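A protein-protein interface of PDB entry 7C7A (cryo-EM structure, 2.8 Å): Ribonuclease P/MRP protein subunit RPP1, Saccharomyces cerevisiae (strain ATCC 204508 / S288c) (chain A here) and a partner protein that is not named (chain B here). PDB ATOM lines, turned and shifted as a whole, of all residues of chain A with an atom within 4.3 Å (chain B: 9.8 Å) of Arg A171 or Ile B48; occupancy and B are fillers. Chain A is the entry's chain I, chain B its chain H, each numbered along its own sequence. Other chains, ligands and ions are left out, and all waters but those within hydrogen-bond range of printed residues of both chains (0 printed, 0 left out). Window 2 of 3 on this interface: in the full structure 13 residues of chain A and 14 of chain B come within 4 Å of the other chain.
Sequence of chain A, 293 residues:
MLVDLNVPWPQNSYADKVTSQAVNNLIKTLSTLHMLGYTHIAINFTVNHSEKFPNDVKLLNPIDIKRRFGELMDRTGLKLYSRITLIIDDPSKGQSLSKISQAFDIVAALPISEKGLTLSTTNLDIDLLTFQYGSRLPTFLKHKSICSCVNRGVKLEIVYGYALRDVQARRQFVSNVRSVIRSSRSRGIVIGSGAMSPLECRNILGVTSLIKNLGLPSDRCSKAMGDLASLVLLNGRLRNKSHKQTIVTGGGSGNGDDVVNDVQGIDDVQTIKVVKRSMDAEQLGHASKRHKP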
ATOM      1  N   VAL A 167      -5.442  31.714  -2.491  1.00  0.00           N
ATOM      2  CA  VAL A 167      -6.818  31.808  -2.958  1.00  0.00           C
ATOM      3  C   VAL A 167      -7.145  30.777  -4.035  1.00  0.00           C
ATOM      4  O   VAL A 167      -8.279  30.274  -4.059  1.00  0.00           O
ATOM      5  CB  VAL A 167      -7.131  33.231  -3.468  1.00  0.00           C
ATOM      6  CG1 VAL A 167      -8.592  33.355  -3.882  1.00  0.00           C
ATOM      7  CG2 VAL A 167      -6.782  34.264  -2.407  1.00  0.00           C
ATOM      8  N   GLN A 168      -6.195  30.429  -4.903  1.00  0.00           N
ATOM      9  CA  GLN A 168      -6.464  29.529  -6.018  1.00  0.00           C
ATOM     10  C   GLN A 168      -6.597  28.073  -5.594  1.00  0.00           C
ATOM     11  O   GLN A 168      -7.486  27.372  -6.094  1.00  0.00           O
ATOM     12  CB  GLN A 168      -5.360  29.655  -7.072  1.00  0.00           C
ATOM     13  CG  GLN A 168      -5.532  28.736  -8.271  1.00  0.00           C
ATOM     14  CD  GLN A 168      -6.756  29.078  -9.098  1.00  0.00           C
ATOM     15  OE1 GLN A 168      -7.669  28.266  -9.243  1.00  0.00           O
ATOM     16  NE2 GLN A 168      -6.780  30.287  -9.646  1.00  0.00           N
ATOM     17  N   ALA A 169      -5.742  27.597  -4.686  1.00  0.00           N
ATOM     18  CA  ALA A 169      -5.803  26.200  -4.271  1.00  0.00           C
ATOM     19  C   ALA A 169      -7.006  25.904  -3.387  1.00  0.00           C
ATOM     20  O   ALA A 169      -7.243  24.737  -3.058  1.00  0.00           O
ATOM     21  CB  ALA A 169      -4.516  25.804  -3.546  1.00  0.00           C
ATOM     22  N   ARG A 170      -7.765  26.930  -2.989  1.00  0.00           N
ATOM     23  CA  ARG A 170      -8.979  26.699  -2.214  1.00  0.00           C
ATOM     24  C   ARG A 170      -9.983  25.867  -3.001  1.00  0.00           C
ATOM     25  O   ARG A 170     -10.648  24.987  -2.443  1.00  0.00           O
ATOM     26  CB  ARG A 170      -9.600  28.033  -1.800  1.00  0.00           C
ATOM     27  CG  ARG A 170      -9.185  28.524  -0.425  1.00  0.00           C
ATOM     28  CD  ARG A 170      -9.778  29.894  -0.139  1.00  0.00           C
ATOM     29  NE  ARG A 170      -9.427  30.381   1.192  1.00  0.00           N
ATOM     30  CZ  ARG A 170      -9.664  31.617   1.619  1.00  0.00           C
ATOM     31  NH1 ARG A 170     -10.257  32.494   0.821  1.00  0.00           N
ATOM     32  NH2 ARG A 170      -9.312  31.975   2.846  1.00  0.00           N
ATOM     33  N   ARG A 171     -10.101  26.132  -4.304  1.00  0.00           N
ATOM     34  CA  ARG A 171     -11.021  25.376  -5.146  1.00  0.00           C
ATOM     35  C   ARG A 171     -10.646  23.901  -5.192  1.00  0.00           C
ATOM     36  O   ARG A 171     -11.511  23.033  -5.030  1.00  0.00           O
ATOM     37  CB  ARG A 171     -11.042  25.960  -6.560  1.00  0.00           C
ATOM     38  CG  ARG A 171     -11.681  27.336  -6.669  1.00  0.00           C
ATOM     39  CD  ARG A 171     -10.662  28.446  -6.454  1.00  0.00           C
ATOM     40  NE  ARG A 171     -11.245  29.772  -6.637  1.00  0.00           N
ATOM     41  CZ  ARG A 171     -11.318  30.401  -7.806  1.00  0.00           C
ATOM     42  NH1 ARG A 171     -10.844  29.823  -8.901  1.00  0.00           N
ATOM     43  NH2 ARG A 171     -11.865  31.606  -7.879  1.00  0.00           N
ATOM     44  N   GLN A 172      -9.362  23.603  -5.408  1.00  0.00           N
ATOM     45  CA  GLN A 172      -8.903  22.221  -5.402  1.00  0.00           C
ATOM     46  C   GLN A 172      -9.077  21.563  -4.041  1.00  0.00           C
ATOM     47  O   GLN A 172      -9.482  20.398  -3.978  1.00  0.00           O
ATOM     48  CB  GLN A 172      -7.436  22.149  -5.830  1.00  0.00           C
ATOM     49  CG  GLN A 172      -7.133  22.861  -7.138  1.00  0.00           C
ATOM     50  CD  GLN A 172      -7.864  22.250  -8.319  1.00  0.00           C
ATOM     51  OE1 GLN A 172      -8.071  21.039  -8.376  1.00  0.00           O
ATOM     52  NE2 GLN A 172      -8.257  23.089  -9.270  1.00  0.00           N
ATOM     53  N   PHE A 173      -8.790  22.282  -2.953  1.00  0.00           N
ATOM     54  CA  PHE A 173      -8.991  21.724  -1.621  1.00  0.00           C
ATOM     55  C   PHE A 173     -10.452  21.369  -1.379  1.00  0.00           C
ATOM     56  O   PHE A 173     -10.749  20.304  -0.827  1.00  0.00           O
ATOM     57  CB  PHE A 173      -8.505  22.705  -0.555  1.00  0.00           C
ATOM     58  CG  PHE A 173      -9.073  22.442   0.811  1.00  0.00           C
ATOM     59  CD1 PHE A 173      -8.612  21.383   1.576  1.00  0.00           C
ATOM     60  CD2 PHE A 173     -10.074  23.249   1.327  1.00  0.00           C
ATOM     61  CE1 PHE A 173      -9.135  21.137   2.831  1.00  0.00           C
ATOM     62  CE2 PHE A 173     -10.600  23.008   2.583  1.00  0.00           C
ATOM     63  CZ  PHE A 173     -10.130  21.951   3.335  1.00  0.00           C
ATOM     64  N   VAL A 174     -11.374  22.244  -1.784  1.00  0.00           N
ATOM     65  CA  VAL A 174     -12.794  21.965  -1.593  1.00  0.00           C
ATOM     66  C   VAL A 174     -13.231  20.791  -2.462  1.00  0.00           C
ATOM     67  O   VAL A 174     -13.957  19.895  -2.006  1.00  0.00           O
ATOM     68  CB  VAL A 174     -13.627  23.228  -1.875  1.00  0.00           C
ATOM     69  CG1 VAL A 174     -15.106  22.892  -1.914  1.00  0.00           C
ATOM     70  CG2 VAL A 174     -13.351  24.289  -0.821  1.00  0.00           C
ATOM     71  N   SER A 175     -12.792  20.768  -3.723  1.00  0.00           N
ATOM     72  CA  SER A 175     -13.129  19.677  -4.628  1.00  0.00           C
ATOM     73  C   SER A 175     -12.562  18.338  -4.178  1.00  0.00           C
ATOM     74  O   SER A 175     -13.136  17.298  -4.517  1.00  0.00           O
ATOM     75  CB  SER A 175     -12.632  19.996  -6.040  1.00  0.00           C
ATOM     76  OG  SER A 175     -12.906  18.928  -6.932  1.00  0.00           O
ATOM     77  N   ASN B  39     -18.586  25.779 -15.000  1.00  0.00           N
ATOM     78  CA  ASN B  39     -17.613  26.434 -14.134  1.00  0.00           C
ATOM     79  C   ASN B  39     -17.881  27.924 -13.996  1.00  0.00           C
ATOM     80  O   ASN B  39     -17.608  28.500 -12.937  1.00  0.00           O
ATOM     81  CB  ASN B  39     -16.198  26.201 -14.667  1.00  0.00           C
ATOM     82  CG  ASN B  39     -15.646  24.843 -14.280  1.00  0.00           C
ATOM     83  OD1 ASN B  39     -15.275  24.042 -15.138  1.00  0.00           O
ATOM     84  ND2 ASN B  39     -15.593  24.575 -12.981  1.00  0.00           N
ATOM     85  N   ALA B  41     -21.065  29.264 -14.330  1.00  0.00           N
ATOM     86  CA  ALA B  41     -22.320  29.368 -13.593  1.00  0.00           C
ATOM     87  C   ALA B  41     -22.092  29.201 -12.097  1.00  0.00           C
ATOM     88  O   ALA B  41     -22.632  29.961 -11.284  1.00  0.00           O
ATOM     89  CB  ALA B  41     -23.313  28.324 -14.106  1.00  0.00           C
ATOM     90  N   LEU B  42     -21.295  28.202 -11.714  1.00  0.00           N
ATOM     91  CA  LEU B  42     -21.047  27.927 -10.305  1.00  0.00           C
ATOM     92  C   LEU B  42     -20.317  29.082  -9.632  1.00  0.00           C
ATOM     93  O   LEU B  42     -20.603  29.415  -8.478  1.00  0.00           O
ATOM     94  CB  LEU B  42     -20.252  26.630 -10.146  1.00  0.00           C
ATOM     95  CG  LEU B  42     -20.988  25.364 -10.591  1.00  0.00           C
ATOM     96  CD1 LEU B  42     -20.060  24.159 -10.606  1.00  0.00           C
ATOM     97  CD2 LEU B  42     -22.197  25.104  -9.705  1.00  0.00           C
ATOM     98  N   LYS B  43     -19.373  29.701 -10.342  1.00  0.00           N
ATOM     99  CA  LYS B  43     -18.596  30.796  -9.773  1.00  0.00           C
ATOM    100  C   LYS B  43     -19.384  32.101  -9.783  1.00  0.00           C
ATOM    101  O   LYS B  43     -19.121  32.993  -8.970  1.00  0.00           O
ATOM    102  CB  LYS B  43     -17.270  30.965 -10.517  1.00  0.00           C
ATOM    103  CG  LYS B  43     -17.380  31.551 -11.911  1.00  0.00           C
ATOM    104  CD  LYS B  43     -16.016  31.603 -12.575  1.00  0.00           C
ATOM    105  CE  LYS B  43     -15.095  32.584 -11.868  1.00  0.00           C
ATOM    106  NZ  LYS B  43     -15.580  33.988 -11.974  1.00  0.00           N
ATOM    107  N   ARG B  44     -20.345  32.233 -10.701  1.00  0.00           N
ATOM    108  CA  ARG B  44     -21.163  33.441 -10.741  1.00  0.00           C
ATOM    109  C   ARG B  44     -22.254  33.409  -9.678  1.00  0.00           C
ATOM    110  O   ARG B  44     -22.464  34.395  -8.965  1.00  0.00           O
ATOM    111  CB  ARG B  44     -21.777  33.619 -12.129  1.00  0.00           C
ATOM    112  CG  ARG B  44     -22.716  34.812 -12.239  1.00  0.00           C
ATOM    113  CD  ARG B  44     -21.955  36.127 -12.292  1.00  0.00           C
ATOM    114  NE  ARG B  44     -21.117  36.226 -13.484  1.00  0.00           N
ATOM    115  CZ  ARG B  44     -21.564  36.589 -14.682  1.00  0.00           C
ATOM    116  NH1 ARG B  44     -22.845  36.886 -14.854  1.00  0.00           N
ATOM    117  NH2 ARG B  44     -20.731  36.653 -15.712  1.00  0.00           N
ATOM    118  N   SER B  45     -22.956  32.284  -9.557  1.00  0.00           N
ATOM    119  CA  SER B  45     -24.027  32.154  -8.578  1.00  0.00           C
ATOM    120  C   SER B  45     -23.525  31.865  -7.172  1.00  0.00           C
ATOM    121  O   SER B  45     -24.136  32.325  -6.201  1.00  0.00           O
ATOM    122  CB  SER B  45     -24.999  31.047  -8.997  1.00  0.00           C
ATOM    123  OG  SER B  45     -24.371  29.774  -8.973  1.00  0.00           O
ATOM    124  N   TYR B  46     -22.434  31.116  -7.038  1.00  0.00           N
ATOM    125  CA  TYR B  46     -21.873  30.755  -5.746  1.00  0.00           C
ATOM    126  C   TYR B  46     -20.395  31.114  -5.713  1.00  0.00           C
ATOM    127  O   TYR B  46     -19.815  31.523  -6.724  1.00  0.00           O
ATOM    128  CB  TYR B  46     -22.045  29.256  -5.458  1.00  0.00           C
ATOM    129  CG  TYR B  46     -23.432  28.843  -5.010  1.00  0.00           C
ATOM    130  CD1 TYR B  46     -23.635  28.255  -3.769  1.00  0.00           C
ATOM    131  CD2 TYR B  46     -24.536  29.027  -5.834  1.00  0.00           C
ATOM    132  CE1 TYR B  46     -24.896  27.869  -3.357  1.00  0.00           C
ATOM    133  CE2 TYR B  46     -25.802  28.646  -5.430  1.00  0.00           C
ATOM    134  CZ  TYR B  46     -25.976  28.067  -4.191  1.00  0.00           C
ATOM    135  OH  TYR B  46     -27.236  27.685  -3.786  1.00  0.00           O
ATOM    136  N   GLY B  47     -19.790  30.968  -4.538  1.00  0.00           N
ATOM    137  CA  GLY B  47     -18.361  31.159  -4.406  1.00  0.00           C
ATOM    138  C   GLY B  47     -17.603  29.861  -4.587  1.00  0.00           C
ATOM    139  O   GLY B  47     -17.874  29.106  -5.524  1.00  0.00           O
ATOM    140  N   ILE B  48     -16.653  29.587  -3.691  1.00  0.00           N
ATOM    141  CA  ILE B  48     -15.931  28.321  -3.737  1.00  0.00           C
ATOM    142  C   ILE B  48     -16.862  27.159  -3.411  1.00  0.00           C
ATOM    143  O   ILE B  48     -16.615  26.016  -3.818  1.00  0.00           O
ATOM    144  CB  ILE B  48     -14.724  28.366  -2.781  1.00  0.00           C
ATOM    145  CG1 ILE B  48     -14.090  29.760  -2.785  1.00  0.00           C
ATOM    146  CG2 ILE B  48     -13.696  27.312  -3.162  1.00  0.00           C
ATOM    147  CD1 ILE B  48     -13.446  30.142  -4.104  1.00  0.00           C
ATOM    148  N   PHE B  49     -17.941  27.435  -2.674  1.00  0.00           N
ATOM    149  CA  PHE B  49     -18.916  26.401  -2.343  1.00  0.00           C
ATOM    150  C   PHE B  49     -19.487  25.763  -3.604  1.00  0.00           C
ATOM    151  O   PHE B  49     -19.526  24.534  -3.730  1.00  0.00           O
ATOM    152  CB  PHE B  49     -20.032  26.998  -1.481  1.00  0.00           C
ATOM    153  CG  PHE B  49     -21.013  25.984  -0.959  1.00  0.00           C
ATOM    154  CD1 PHE B  49     -22.138  25.641  -1.694  1.00  0.00           C
ATOM    155  CD2 PHE B  49     -20.818  25.384   0.273  1.00  0.00           C
ATOM    156  CE1 PHE B  49     -23.042  24.712  -1.214  1.00  0.00           C
ATOM    157  CE2 PHE B  49     -21.717  24.453   0.759  1.00  0.00           C
ATOM    158  CZ  PHE B  49     -22.831  24.117   0.015  1.00  0.00           C
ATOM    159  N   GLY B  50     -19.934  26.588  -4.552  1.00  0.00           N
ATOM    160  CA  GLY B  50     -20.453  26.051  -5.798  1.00  0.00           C
ATOM    161  C   GLY B  50     -19.371  25.515  -6.713  1.00  0.00           C
ATOM    162  O   GLY B  50     -19.611  24.581  -7.482  1.00  0.00           O
ATOM    163  N   GLU B  51     -18.167  26.088  -6.643  1.00  0.00           N
ATOM    164  CA  GLU B  51     -17.071  25.636  -7.490  1.00  0.00           C
ATOM    165  C   GLU B  51     -16.544  24.266  -7.089  1.00  0.00           C
ATOM    166  O   GLU B  51     -16.022  23.544  -7.946  1.00  0.00           O
ATOM    167  CB  GLU B  51     -15.926  26.650  -7.460  1.00  0.00           C
ATOM    168  CG  GLU B  51     -16.267  27.998  -8.074  1.00  0.00           C
ATOM    169  CD  GLU B  51     -15.036  28.834  -8.360  1.00  0.00           C
ATOM    170  OE1 GLU B  51     -15.127  30.077  -8.283  1.00  0.00           O
ATOM    171  OE2 GLU B  51     -13.979  28.248  -8.670  1.00  0.00           O
ATOM    172  N   GLY B  52     -16.666  23.892  -5.819  1.00  0.00           N
ATOM    173  CA  GLY B  52     -16.170  22.607  -5.366  1.00  0.00           C
ATOM    174  C   GLY B  52     -17.159  21.471  -5.531  1.00  0.00           C
ATOM    175  O   GLY B  52     -16.996  20.407  -4.926  1.00  0.00           O
ATOM    176  N   VAL B  53     -18.188  21.678  -6.352  1.00  0.00           N
ATOM    177  CA  VAL B  53     -19.194  20.646  -6.569  1.00  0.00           C
ATOM    178  C   VAL B  53     -18.661  19.624  -7.564  1.00  0.00           C
ATOM    179  O   VAL B  53     -18.128  19.981  -8.623  1.00  0.00           O
ATOM    180  CB  VAL B  53     -20.510  21.271  -7.055  1.00  0.00           C
ATOM    181  CG1 VAL B  53     -21.468  20.194  -7.544  1.00  0.00           C
ATOM    182  CG2 VAL B  53     -21.148  22.092  -5.944  1.00  0.00           C
ATOM    183  N   GLU B  54     -18.796  18.344  -7.224  1.00  0.00           N
ATOM    184  CA  GLU B  54     -18.321  17.267  -8.085  1.00  0.00           C
ATOM    185  C   GLU B  54     -19.356  16.972  -9.165  1.00  0.00           C
ATOM    186  O   GLU B  54     -20.540  16.789  -8.863  1.00  0.00           O
ATOM    187  CB  GLU B  54     -18.031  16.014  -7.261  1.00  0.00           C
ATOM    188  CG  GLU B  54     -17.485  14.851  -8.074  1.00  0.00           C
ATOM    189  CD  GLU B  54     -17.195  13.631  -7.221  1.00  0.00           C
ATOM    190  OE1 GLU B  54     -17.434  13.690  -5.997  1.00  0.00           O
ATOM    191  OE2 GLU B  54     -16.731  12.613  -7.777  1.00  0.00           O
ATOM    192  N   TYR B  55     -18.909  16.924 -10.419  1.00  0.00           N
ATOM    193  CA  TYR B  55     -19.771  16.611 -11.549  1.00  0.00           C
ATOM    194  C   TYR B  55     -18.921  16.108 -12.707  1.00  0.00           C
ATOM    195  O   TYR B  55     -17.815  16.604 -12.935  1.00  0.00           O
ATOM    196  CB  TYR B  55     -20.594  17.833 -11.987  1.00  0.00           C
ATOM    197  CG  TYR B  55     -19.764  19.026 -12.416  1.00  0.00           C
ATOM    198  CD1 TYR B  55     -19.336  19.968 -11.490  1.00  0.00           C
ATOM    199  CD2 TYR B  55     -19.420  19.217 -13.749  1.00  0.00           C
ATOM    200  CE1 TYR B  55     -18.578  21.061 -11.877  1.00  0.00           C
ATOM    201  CE2 TYR B  55     -18.663  20.304 -14.144  1.00  0.00           C
ATOM    202  CZ  TYR B  55     -18.246  21.224 -13.206  1.00  0.00           C
ATOM    203  OH  TYR B  55     -17.494  22.307 -13.601  1.00  0.00           O
ATOM    204  N   ASP B  73     -25.538  17.358  -2.842  1.00  0.00           N
ATOM    205  CA  ASP B  73     -25.385  18.618  -3.561  1.00  0.00           C
ATOM    206  C   ASP B  73     -26.414  18.765  -4.677  1.00  0.00           C
ATOM    207  O   ASP B  73     -26.254  19.609  -5.566  1.00  0.00           O
ATOM    208  CB  ASP B  73     -23.971  18.733  -4.135  1.00  0.00           C
ATOM    209  CG  ASP B  73     -22.918  18.920  -3.060  1.00  0.00           C
ATOM    210  OD1 ASP B  73     -23.241  19.503  -2.004  1.00  0.00           O
ATOM    211  OD2 ASP B  73     -21.765  18.485  -3.272  1.00  0.00           O
ATOM    212  N   THR B  76     -27.850  22.311  -4.331  1.00  0.00           N
ATOM    213  CA  THR B  76     -26.922  23.316  -4.839  1.00  0.00           C
ATOM    214  C   THR B  76     -26.862  23.290  -6.363  1.00  0.00           C
ATOM    215  O   THR B  76     -26.768  24.341  -7.008  1.00  0.00           O
ATOM    216  CB  THR B  76     -25.530  23.098  -4.238  1.00  0.00           C
ATOM    217  OG1 THR B  76     -25.588  23.260  -2.815  1.00  0.00           O
ATOM    218  CG2 THR B  76     -24.525  24.090  -4.812  1.00  0.00           C
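Of the 9 printed residues of chain A, 4 touch a printed residue of chain B. Hydrophobic or aromatic side chains of chain B that line the printed part of chain A: Ile B48. Among the printed residues, 6 pairs touch across the chains. Among the printed residues, Asp or Glu carboxylates within 4 Å of a Lys or Arg side-chain nitrogen of the other chain: Arg A171 with Glu B51 (3.5 Å).
Among the printed residues, merely in contact across the chains: Arg A171 with Ile B48 (3.4 Å), Val A174 with Gly B52 (3.6 Å), Val A174 with Ile B48 (3.8 Å), Arg A170 with Ile B48 (3.9 Å) and Ser A175 with Gly B52 (3.9 Å).
Of chain B, only Ile B48 and Glu B51 come within 4 Å of Arg A171. Of chain A, only Arg A170 (3.9 Å), Arg A171 (3.4 Å) and Val A174 (3.8 Å) come within 4 Å of Ile B48. No residue of chain B comes within 4 Å of Ala A169. Of chain B, only Ile B48 (3.8 Å) and Gly B52 (3.6 Å) come within 4 Å of Val A174. Of the printed residues of chain A, Gly B52 touches Val A174 and Ser A175. Printed residues of chain B within 4 Å of Arg A170: Ile B48. Printed residues of chain B within 4 Å of Ser A175: Gly B52 (3.9 Å). Of the printed residues of chain A, Glu B51 touches Arg A171. The nearest printed residue of chain A that does not touch Ile B48 is Val A167 (5.2 Å). The nearest printed residue of chain B that does not touch Arg A170 is Gly B52 (6.7 Å).
OE2 of Glu B51 lies within salt-bridge range of NH1 of Arg A171, 3.5 Å away.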
